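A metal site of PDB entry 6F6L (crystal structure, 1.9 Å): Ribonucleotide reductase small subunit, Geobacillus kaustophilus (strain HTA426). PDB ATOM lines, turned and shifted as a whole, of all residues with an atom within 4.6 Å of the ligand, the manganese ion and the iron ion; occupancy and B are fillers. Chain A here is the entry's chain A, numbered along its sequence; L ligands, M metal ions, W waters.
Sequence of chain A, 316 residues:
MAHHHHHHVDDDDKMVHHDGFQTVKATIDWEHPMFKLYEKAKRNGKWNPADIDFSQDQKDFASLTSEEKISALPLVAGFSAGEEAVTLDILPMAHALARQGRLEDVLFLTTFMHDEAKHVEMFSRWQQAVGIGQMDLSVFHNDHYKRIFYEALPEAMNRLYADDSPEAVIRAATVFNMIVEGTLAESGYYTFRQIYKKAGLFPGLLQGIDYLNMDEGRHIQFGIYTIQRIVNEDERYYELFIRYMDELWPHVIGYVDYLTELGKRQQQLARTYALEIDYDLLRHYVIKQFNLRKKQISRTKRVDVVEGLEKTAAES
The backbone carbonyl oxygen (O) of Ser 187 lies within hydrogen-bond range of the side-chain hydroxyl (OG1) of Thr 191, at 2.8 Å.
The backbone carbonyl oxygen (O) of Val 256 sits at hydrogen-bond distance from the side-chain hydroxyl (OG1) of Thr 260 (3.0 Å).
The backbone NH (N) of Ala 185 lies within hydrogen-bond range of the backbone carbonyl oxygen (O) of Val 180, 2.8 Å away.
Gly 78 touches the ligand (C to C7, 3.5 Å).
Phe 79 touches the ligand.
CA of Gly 82 touches C4 of the ligand, 3.97 Å away.
CG2 of Val 86 touches C1 of the ligand, 3.8 Å away.
CZ of Phe 149 touches C6 of the ligand (3.7 Å).
Val 180 touches the ligand.
O of Leu 184 touches C10 of the ligand (3.7 Å).
Ala 185 touches the ligand (CB to C3, 3.99 Å).
Gly 188 touches the ligand (CA to C11, 3.7 Å).
Thr 191 touches the ligand.
CE2 of Tyr 255 touches C10 of the ligand, 3.9 Å away.
CG2 of Val 256 touches C12 of the ligand, 3.9 Å away.
Leu 259 touches the ligand (CD1 to C14, 3.8 Å).
OG1 of Thr 260 touches C16 of the ligand, at 3.98 Å.
Within 4 Å of the ligand: Gly 78, Phe 79, Gly 82, Glu 83, Val 86, Glu 116, His 119, Phe 149, Val 180, Glu 181, Leu 184, Ala 185, Gly 188, Thr 191, Glu 216, Tyr 255, Val 256, Leu 259 and Thr 260.
The nearest printed residue that does not touch the iron ion is Phe 112 (4.03 Å).
The manganese ion is bound by O1 of the ligand (1.7 Å), OE1 of Glu 116 (2.1 Å), OE1 of Glu 83 (2.1 Å), ND1 of His 119 (2.1 Å), water W2 (2.2 Å) and water W1 (2.3 Å).
The manganese ion has six donor atoms within binding distance.
OE2 of Glu 181 is bound to the iron ion (2.0 Å).
Water W2 is bound to the iron ion (2.1 Å).
The iron ion is bound by the side-chain carboxylate (OE2) of Glu 116, 2.1 Å away.
O2 of the ligand is bound to the iron ion.
The iron ion is bound by OE2 of Glu 216 (2.2 Å).
A ring nitrogen (ND1) of His 219 is bound to the iron ion, at 2.3 Å.
Water W1 bridges the side-chain hydroxyl of Tyr 189 (2.6 Å) and the side-chain carboxylate of Glu 216 (3.1 Å).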
ATOM      1  N   LEU A  75      -5.629  19.808  36.847  1.00  0.00           N
ATOM      2  CA  LEU A  75      -5.630  20.980  35.976  1.00  0.00           C
ATOM      3  C   LEU A  75      -4.577  20.864  34.888  1.00  0.00           C
ATOM      4  O   LEU A  75      -4.838  21.177  33.732  1.00  0.00           O
ATOM      5  CB  LEU A  75      -5.390  22.237  36.804  1.00  0.00           C
ATOM      6  CG  LEU A  75      -6.277  23.431  36.469  1.00  0.00           C
ATOM      7  CD1 LEU A  75      -7.727  23.115  36.858  1.00  0.00           C
ATOM      8  CD2 LEU A  75      -5.764  24.676  37.212  1.00  0.00           C
ATOM      9  N   GLY A  78      -5.577  18.443  32.205  1.00  0.00           N
ATOM     10  CA  GLY A  78      -6.561  18.937  31.259  1.00  0.00           C
ATOM     11  C   GLY A  78      -5.933  19.847  30.239  1.00  0.00           C
ATOM     12  O   GLY A  78      -6.261  19.802  29.045  1.00  0.00           O
ATOM     13  N   PHE A  79      -5.034  20.718  30.697  1.00  0.00           N
ATOM     14  CA  PHE A  79      -4.337  21.603  29.774  1.00  0.00           C
ATOM     15  C   PHE A  79      -3.427  20.832  28.840  1.00  0.00           C
ATOM     16  O   PHE A  79      -3.368  21.148  27.655  1.00  0.00           O
ATOM     17  CB  PHE A  79      -3.524  22.635  30.517  1.00  0.00           C
ATOM     18  CG  PHE A  79      -4.261  23.920  30.742  1.00  0.00           C
ATOM     19  CD1 PHE A  79      -4.479  24.798  29.696  1.00  0.00           C
ATOM     20  CD2 PHE A  79      -4.769  24.222  31.995  1.00  0.00           C
ATOM     21  CE1 PHE A  79      -5.173  25.966  29.913  1.00  0.00           C
ATOM     22  CE2 PHE A  79      -5.466  25.426  32.218  1.00  0.00           C
ATOM     23  CZ  PHE A  79      -5.670  26.269  31.178  1.00  0.00           C
ATOM     24  N   GLY A  82      -5.377  19.224  26.236  1.00  0.00           N
ATOM     25  CA  GLY A  82      -6.028  20.278  25.485  1.00  0.00           C
ATOM     26  C   GLY A  82      -5.117  20.937  24.461  1.00  0.00           C
ATOM     27  O   GLY A  82      -5.495  21.101  23.294  1.00  0.00           O
ATOM     28  N   GLU A  83      -3.905  21.354  24.885  1.00  0.00           N
ATOM     29  CA  GLU A  83      -2.954  21.985  23.964  1.00  0.00           C
ATOM     30  C   GLU A  83      -2.582  21.029  22.849  1.00  0.00           C
ATOM     31  O   GLU A  83      -2.448  21.426  21.678  1.00  0.00           O
ATOM     32  CB  GLU A  83      -1.673  22.418  24.706  1.00  0.00           C
ATOM     33  CG  GLU A  83      -1.861  23.279  25.948  1.00  0.00           C
ATOM     34  CD  GLU A  83      -2.538  24.621  25.696  1.00  0.00           C
ATOM     35  OE1 GLU A  83      -2.662  25.022  24.514  1.00  0.00           O
ATOM     36  OE2 GLU A  83      -2.943  25.263  26.695  1.00  0.00           O
ATOM     37  N   VAL A  86      -5.568  20.674  20.353  1.00  0.00           N
ATOM     38  CA  VAL A  86      -5.784  21.819  19.459  1.00  0.00           C
ATOM     39  C   VAL A  86      -4.602  22.000  18.502  1.00  0.00           C
ATOM     40  O   VAL A  86      -4.787  22.495  17.383  1.00  0.00           O
ATOM     41  CB  VAL A  86      -6.066  23.126  20.250  1.00  0.00           C
ATOM     42  CG1 VAL A  86      -7.380  23.003  21.060  1.00  0.00           C
ATOM     43  CG2 VAL A  86      -4.898  23.500  21.134  1.00  0.00           C
ATOM     44  N   PHE A 112      -1.255  30.916  14.974  1.00  0.00           N
ATOM     45  CA  PHE A 112      -2.136  30.193  15.889  1.00  0.00           C
ATOM     46  C   PHE A 112      -1.583  28.800  16.156  1.00  0.00           C
ATOM     47  O   PHE A 112      -1.412  28.391  17.316  1.00  0.00           O
ATOM     48  CB  PHE A 112      -3.530  30.148  15.232  1.00  0.00           C
ATOM     49  CG  PHE A 112      -4.651  29.687  16.107  1.00  0.00           C
ATOM     50  CD1 PHE A 112      -5.928  30.122  15.839  1.00  0.00           C
ATOM     51  CD2 PHE A 112      -4.485  28.759  17.106  1.00  0.00           C
ATOM     52  CE1 PHE A 112      -6.973  29.732  16.605  1.00  0.00           C
ATOM     53  CE2 PHE A 112      -5.558  28.336  17.864  1.00  0.00           C
ATOM     54  CZ  PHE A 112      -6.793  28.799  17.624  1.00  0.00           C
ATOM     55  N   GLU A 116       0.139  27.135  19.657  1.00  0.00           N
ATOM     56  CA  GLU A 116      -0.304  25.947  20.354  1.00  0.00           C
ATOM     57  C   GLU A 116       0.847  24.966  20.524  1.00  0.00           C
ATOM     58  O   GLU A 116       0.952  24.274  21.565  1.00  0.00           O
ATOM     59  CB  GLU A 116      -1.498  25.276  19.660  1.00  0.00           C
ATOM     60  CG  GLU A 116      -2.724  26.154  19.457  1.00  0.00           C
ATOM     61  CD  GLU A 116      -3.406  26.584  20.738  1.00  0.00           C
ATOM     62  OE1 GLU A 116      -2.915  26.284  21.872  1.00  0.00           O
ATOM     63  OE2 GLU A 116      -4.496  27.168  20.599  1.00  0.00           O
ATOM     64  N   HIS A 119       2.512  25.978  23.457  1.00  0.00           N
ATOM     65  CA  HIS A 119       1.762  25.672  24.669  1.00  0.00           C
ATOM     66  C   HIS A 119       1.951  24.218  25.102  1.00  0.00           C
ATOM     67  O   HIS A 119       2.053  23.936  26.303  1.00  0.00           O
ATOM     68  CB  HIS A 119       0.289  25.942  24.453  1.00  0.00           C
ATOM     69  CG  HIS A 119       0.007  27.374  24.121  1.00  0.00           C
ATOM     70  ND1 HIS A 119      -1.271  27.854  23.937  1.00  0.00           N
ATOM     71  CD2 HIS A 119       0.835  28.424  23.944  1.00  0.00           C
ATOM     72  CE1 HIS A 119      -1.211  29.151  23.667  1.00  0.00           C
ATOM     73  NE2 HIS A 119       0.066  29.519  23.639  1.00  0.00           N
ATOM     74  N   PHE A 149     -12.733  16.597  24.205  1.00  0.00           N
ATOM     75  CA  PHE A 149     -11.383  16.659  23.636  1.00  0.00           C
ATOM     76  C   PHE A 149     -10.973  15.412  22.865  1.00  0.00           C
ATOM     77  O   PHE A 149     -10.222  15.519  21.900  1.00  0.00           O
ATOM     78  CB  PHE A 149     -10.359  16.901  24.742  1.00  0.00           C
ATOM     79  CG  PHE A 149     -10.395  18.302  25.290  1.00  0.00           C
ATOM     80  CD1 PHE A 149      -9.717  19.321  24.665  1.00  0.00           C
ATOM     81  CD2 PHE A 149     -11.136  18.600  26.422  1.00  0.00           C
ATOM     82  CE1 PHE A 149      -9.740  20.608  25.146  1.00  0.00           C
ATOM     83  CE2 PHE A 149     -11.182  19.905  26.898  1.00  0.00           C
ATOM     84  CZ  PHE A 149     -10.462  20.893  26.260  1.00  0.00           C
ATOM     85  N   VAL A 180     -13.699  25.278  23.888  1.00  0.00           N
ATOM     86  CA  VAL A 180     -12.387  24.817  24.360  1.00  0.00           C
ATOM     87  C   VAL A 180     -11.532  25.989  24.832  1.00  0.00           C
ATOM     88  O   VAL A 180     -10.996  25.986  25.953  1.00  0.00           O
ATOM     89  CB  VAL A 180     -11.708  23.985  23.277  1.00  0.00           C
ATOM     90  CG1 VAL A 180     -10.186  23.766  23.583  1.00  0.00           C
ATOM     91  CG2 VAL A 180     -12.452  22.672  23.146  1.00  0.00           C
ATOM     92  N   GLU A 181     -11.357  26.998  23.984  1.00  0.00           N
ATOM     93  CA  GLU A 181     -10.493  28.131  24.292  1.00  0.00           C
ATOM     94  C   GLU A 181     -11.222  29.206  25.113  1.00  0.00           C
ATOM     95  O   GLU A 181     -10.766  29.577  26.199  1.00  0.00           O
ATOM     96  CB  GLU A 181      -9.969  28.742  22.979  1.00  0.00           C
ATOM     97  CG  GLU A 181      -8.890  27.879  22.331  1.00  0.00           C
ATOM     98  CD  GLU A 181      -8.409  28.413  21.014  1.00  0.00           C
ATOM     99  OE1 GLU A 181      -9.271  28.943  20.277  1.00  0.00           O
ATOM    100  OE2 GLU A 181      -7.178  28.320  20.736  1.00  0.00           O
ATOM    101  N   LEU A 184     -13.234  26.952  28.415  1.00  0.00           N
ATOM    102  CA  LEU A 184     -12.469  26.109  29.332  1.00  0.00           C
ATOM    103  C   LEU A 184     -11.058  26.651  29.569  1.00  0.00           C
ATOM    104  O   LEU A 184     -10.644  26.784  30.724  1.00  0.00           O
ATOM    105  CB  LEU A 184     -12.424  24.668  28.813  1.00  0.00           C
ATOM    106  CG  LEU A 184     -13.727  23.900  28.964  1.00  0.00           C
ATOM    107  CD1 LEU A 184     -13.624  22.642  28.112  1.00  0.00           C
ATOM    108  CD2 LEU A 184     -13.995  23.560  30.418  1.00  0.00           C
ATOM    109  N   ALA A 185     -10.321  27.017  28.515  1.00  0.00           N
ATOM    110  CA  ALA A 185      -8.946  27.490  28.725  1.00  0.00           C
ATOM    111  C   ALA A 185      -8.924  28.778  29.556  1.00  0.00           C
ATOM    112  O   ALA A 185      -8.091  28.926  30.474  1.00  0.00           O
ATOM    113  CB  ALA A 185      -8.239  27.731  27.394  1.00  0.00           C
ATOM    114  N   SER A 187     -11.064  29.813  31.792  1.00  0.00           N
ATOM    115  CA  SER A 187     -11.411  29.518  33.170  1.00  0.00           C
ATOM    116  C   SER A 187     -10.286  28.776  33.862  1.00  0.00           C
ATOM    117  O   SER A 187     -10.078  28.985  35.060  1.00  0.00           O
ATOM    118  CB  SER A 187     -12.716  28.712  33.216  1.00  0.00           C
ATOM    119  OG  SER A 187     -13.760  29.428  32.562  1.00  0.00           O
ATOM    120  N   GLY A 188      -9.531  27.949  33.126  1.00  0.00           N
ATOM    121  CA  GLY A 188      -8.316  27.350  33.662  1.00  0.00           C
ATOM    122  C   GLY A 188      -7.227  28.362  34.005  1.00  0.00           C
ATOM    123  O   GLY A 188      -6.537  28.211  35.031  1.00  0.00           O
ATOM    124  N   TYR A 189      -7.002  29.355  33.143  1.00  0.00           N
ATOM    125  CA  TYR A 189      -6.033  30.402  33.468  1.00  0.00           C
ATOM    126  C   TYR A 189      -6.438  31.095  34.765  1.00  0.00           C
ATOM    127  O   TYR A 189      -5.594  31.343  35.633  1.00  0.00           O
ATOM    128  CB  TYR A 189      -5.945  31.465  32.373  1.00  0.00           C
ATOM    129  CG  TYR A 189      -5.568  30.938  31.029  1.00  0.00           C
ATOM    130  CD1 TYR A 189      -4.700  29.893  30.909  1.00  0.00           C
ATOM    131  CD2 TYR A 189      -6.120  31.465  29.872  1.00  0.00           C
ATOM    132  CE1 TYR A 189      -4.370  29.378  29.657  1.00  0.00           C
ATOM    133  CE2 TYR A 189      -5.808  30.948  28.637  1.00  0.00           C
ATOM    134  CZ  TYR A 189      -4.928  29.912  28.536  1.00  0.00           C
ATOM    135  OH  TYR A 189      -4.602  29.368  27.301  1.00  0.00           O
ATOM    136  N   THR A 191      -8.355  29.931  37.164  1.00  0.00           N
ATOM    137  CA  THR A 191      -8.213  28.996  38.260  1.00  0.00           C
ATOM    138  C   THR A 191      -6.762  28.901  38.728  1.00  0.00           C
ATOM    139  O   THR A 191      -6.485  28.891  39.940  1.00  0.00           O
ATOM    140  CB  THR A 191      -8.750  27.622  37.849  1.00  0.00           C
ATOM    141  OG1 THR A 191     -10.145  27.715  37.543  1.00  0.00           O
ATOM    142  CG2 THR A 191      -8.544  26.567  38.941  1.00  0.00           C
ATOM    143  N   GLU A 216      -3.984  33.384  23.773  1.00  0.00           N
ATOM    144  CA  GLU A 216      -5.386  32.947  23.673  1.00  0.00           C
ATOM    145  C   GLU A 216      -6.289  34.049  23.172  1.00  0.00           C
ATOM    146  O   GLU A 216      -7.291  33.779  22.509  1.00  0.00           O
ATOM    147  CB  GLU A 216      -5.903  32.509  25.033  1.00  0.00           C
ATOM    148  CG  GLU A 216      -6.964  31.453  25.017  1.00  0.00           C
ATOM    149  CD  GLU A 216      -6.376  30.205  24.463  1.00  0.00           C
ATOM    150  OE1 GLU A 216      -5.742  29.491  25.229  1.00  0.00           O
ATOM    151  OE2 GLU A 216      -6.498  29.998  23.230  1.00  0.00           O
ATOM    152  N   HIS A 219      -6.508  33.842  19.599  1.00  0.00           N
ATOM    153  CA  HIS A 219      -7.199  32.627  19.168  1.00  0.00           C
ATOM    154  C   HIS A 219      -8.706  32.795  19.242  1.00  0.00           C
ATOM    155  O   HIS A 219      -9.431  32.410  18.312  1.00  0.00           O
ATOM    156  CB  HIS A 219      -6.749  31.431  20.022  1.00  0.00           C
ATOM    157  CG  HIS A 219      -5.272  31.181  19.964  1.00  0.00           C
ATOM    158  ND1 HIS A 219      -4.639  30.136  20.603  1.00  0.00           N
ATOM    159  CD2 HIS A 219      -4.290  31.882  19.350  1.00  0.00           C
ATOM    160  CE1 HIS A 219      -3.336  30.218  20.398  1.00  0.00           C
ATOM    161  NE2 HIS A 219      -3.103  31.265  19.626  1.00  0.00           N
ATOM    162  N   TYR A 255     -17.268  18.447  33.304  1.00  0.00           N
ATOM    163  CA  TYR A 255     -15.829  18.410  33.607  1.00  0.00           C
ATOM    164  C   TYR A 255     -15.531  19.306  34.793  1.00  0.00           C
ATOM    165  O   TYR A 255     -14.850  18.874  35.740  1.00  0.00           O
ATOM    166  CB  TYR A 255     -15.025  18.829  32.374  1.00  0.00           C
ATOM    167  CG  TYR A 255     -13.541  18.909  32.593  1.00  0.00           C
ATOM    168  CD1 TYR A 255     -12.830  17.819  33.058  1.00  0.00           C
ATOM    169  CD2 TYR A 255     -12.857  20.053  32.291  1.00  0.00           C
ATOM    170  CE1 TYR A 255     -11.473  17.875  33.233  1.00  0.00           C
ATOM    171  CE2 TYR A 255     -11.470  20.142  32.489  1.00  0.00           C
ATOM    172  CZ  TYR A 255     -10.798  19.040  32.953  1.00  0.00           C
ATOM    173  OH  TYR A 255      -9.431  19.104  33.133  1.00  0.00           O
ATOM    174  N   VAL A 256     -16.107  20.513  34.818  1.00  0.00           N
ATOM    175  CA  VAL A 256     -15.817  21.476  35.874  1.00  0.00           C
ATOM    176  C   VAL A 256     -16.260  20.940  37.235  1.00  0.00           C
ATOM    177  O   VAL A 256     -15.534  21.035  38.215  1.00  0.00           O
ATOM    178  CB  VAL A 256     -16.489  22.823  35.528  1.00  0.00           C
ATOM    179  CG1 VAL A 256     -16.605  23.698  36.722  1.00  0.00           C
ATOM    180  CG2 VAL A 256     -15.697  23.537  34.434  1.00  0.00           C
ATOM    181  N   LEU A 259     -13.642  18.361  38.336  1.00  0.00           N
ATOM    182  CA  LEU A 259     -12.481  19.011  38.936  1.00  0.00           C
ATOM    183  C   LEU A 259     -12.810  19.587  40.299  1.00  0.00           C
ATOM    184  O   LEU A 259     -11.975  19.536  41.211  1.00  0.00           O
ATOM    185  CB  LEU A 259     -11.969  20.131  38.045  1.00  0.00           C
ATOM    186  CG  LEU A 259     -11.333  19.694  36.729  1.00  0.00           C
ATOM    187  CD1 LEU A 259     -10.984  20.947  35.936  1.00  0.00           C
ATOM    188  CD2 LEU A 259     -10.113  18.845  36.975  1.00  0.00           C
ATOM    189  N   THR A 260     -14.001  20.194  40.432  1.00  0.00           N
ATOM    190  CA  THR A 260     -14.396  20.822  41.681  1.00  0.00           C
ATOM    191  C   THR A 260     -14.507  19.793  42.785  1.00  0.00           C
ATOM    192  O   THR A 260     -14.119  20.051  43.938  1.00  0.00           O
ATOM    193  CB  THR A 260     -15.731  21.531  41.502  1.00  0.00           C
ATOM    194  OG1 THR A 260     -15.549  22.684  40.675  1.00  0.00           O
ATOM    195  CG2 THR A 260     -16.269  21.987  42.810  1.00  0.00           C
ATOM    196  N   TYR A 279     -14.561  27.414  45.428  1.00  0.00           N
ATOM    197  CA  TYR A 279     -14.910  26.619  44.252  1.00  0.00           C
ATOM    198  C   TYR A 279     -16.216  27.084  43.629  1.00  0.00           C
ATOM    199  O   TYR A 279     -16.447  26.837  42.444  1.00  0.00           O
ATOM    200  CB  TYR A 279     -15.007  25.142  44.601  1.00  0.00           C
ATOM    201  CG  TYR A 279     -13.657  24.534  44.759  1.00  0.00           C
ATOM    202  CD1 TYR A 279     -12.839  24.325  43.661  1.00  0.00           C
ATOM    203  CD2 TYR A 279     -13.162  24.209  46.023  1.00  0.00           C
ATOM    204  CE1 TYR A 279     -11.572  23.799  43.806  1.00  0.00           C
ATOM    205  CE2 TYR A 279     -11.903  23.676  46.176  1.00  0.00           C
ATOM    206  CZ  TYR A 279     -11.107  23.471  45.075  1.00  0.00           C
ATOM    207  OH  TYR A 279      -9.849  22.944  45.221  1.00  0.00           O
ATOM    208  N   LEU A 282     -15.255  29.864  41.280  1.00  0.00           N
ATOM    209  CA  LEU A 282     -14.678  29.294  40.065  1.00  0.00           C
ATOM    210  C   LEU A 282     -15.772  28.820  39.124  1.00  0.00           C
ATOM    211  O   LEU A 282     -15.769  29.172  37.933  1.00  0.00           O
ATOM    212  CB  LEU A 282     -13.726  28.151  40.402  1.00  0.00           C
ATOM    213  CG  LEU A 282     -12.516  28.621  41.239  1.00  0.00           C
ATOM    214  CD1 LEU A 282     -11.613  27.468  41.706  1.00  0.00           C
ATOM    215  CD2 LEU A 282     -11.676  29.664  40.495  1.00  0.00           C
ATOM    216  N   VAL A 286     -16.792  30.014  35.078  1.00  0.00           N
ATOM    217  CA  VAL A 286     -17.055  29.179  33.898  1.00  0.00           C
ATOM    218  C   VAL A 286     -18.378  29.584  33.252  1.00  0.00           C
ATOM    219  O   VAL A 286     -18.471  29.752  32.026  1.00  0.00           O
ATOM    220  CB  VAL A 286     -17.054  27.693  34.283  1.00  0.00           C
ATOM    221  CG1 VAL A 286     -17.505  26.814  33.111  1.00  0.00           C
ATOM    222  CG2 VAL A 286     -15.673  27.297  34.726  1.00  0.00           C
HETATM  223  C1  LIG L   1      -5.922  26.099  23.719  1.00  0.00           C
HETATM  224  O1  LIG L   1      -4.760  26.245  24.142  1.00  0.00           O
HETATM  225  O2  LIG L   1      -6.409  26.631  22.716  1.00  0.00           O
HETATM  226  C2  LIG L   1      -6.919  25.181  24.525  1.00  0.00           C
HETATM  227  C3  LIG L   1      -6.462  24.525  25.824  1.00  0.00           C
HETATM  228  C4  LIG L   1      -7.620  23.749  26.555  1.00  0.00           C
HETATM  229  C5  LIG L   1      -7.449  23.592  28.090  1.00  0.00           C
HETATM  230  C6  LIG L   1      -8.525  22.754  28.782  1.00  0.00           C
HETATM  231  C7  LIG L   1      -8.266  22.437  30.297  1.00  0.00           C
HETATM  232  C8  LIG L   1      -8.608  23.596  31.176  1.00  0.00           C
HETATM  233  C9  LIG L   1      -9.089  23.263  32.584  1.00  0.00           C
HETATM  234  C10 LIG L   1     -10.485  23.843  32.886  1.00  0.00           C
HETATM  235  C11 LIG L   1     -10.586  24.495  34.203  1.00  0.00           C
HETATM  236  C12 LIG L   1     -12.016  24.746  34.626  1.00  0.00           C
HETATM  237  C13 LIG L   1     -12.102  25.261  36.062  1.00  0.00           C
HETATM  238  C14 LIG L   1     -12.455  24.222  37.111  1.00  0.00           C
HETATM  239  C15 LIG L   1     -12.548  24.792  38.545  1.00  0.00           C
HETATM  240  C16 LIG L   1     -11.901  23.912  39.654  1.00  0.00           C
HETATM  241 MN    MN M   1      -3.198  26.925  23.827  1.00  0.00          MN
HETATM  242 FE    FE M   2      -5.536  28.496  21.893  1.00  0.00          FE
HETATM  243  O   HOH W   1      -3.642  27.312  26.061  1.00  0.00           O
HETATM  244  O   HOH W   2      -4.034  28.874  23.276  1.00  0.00           O
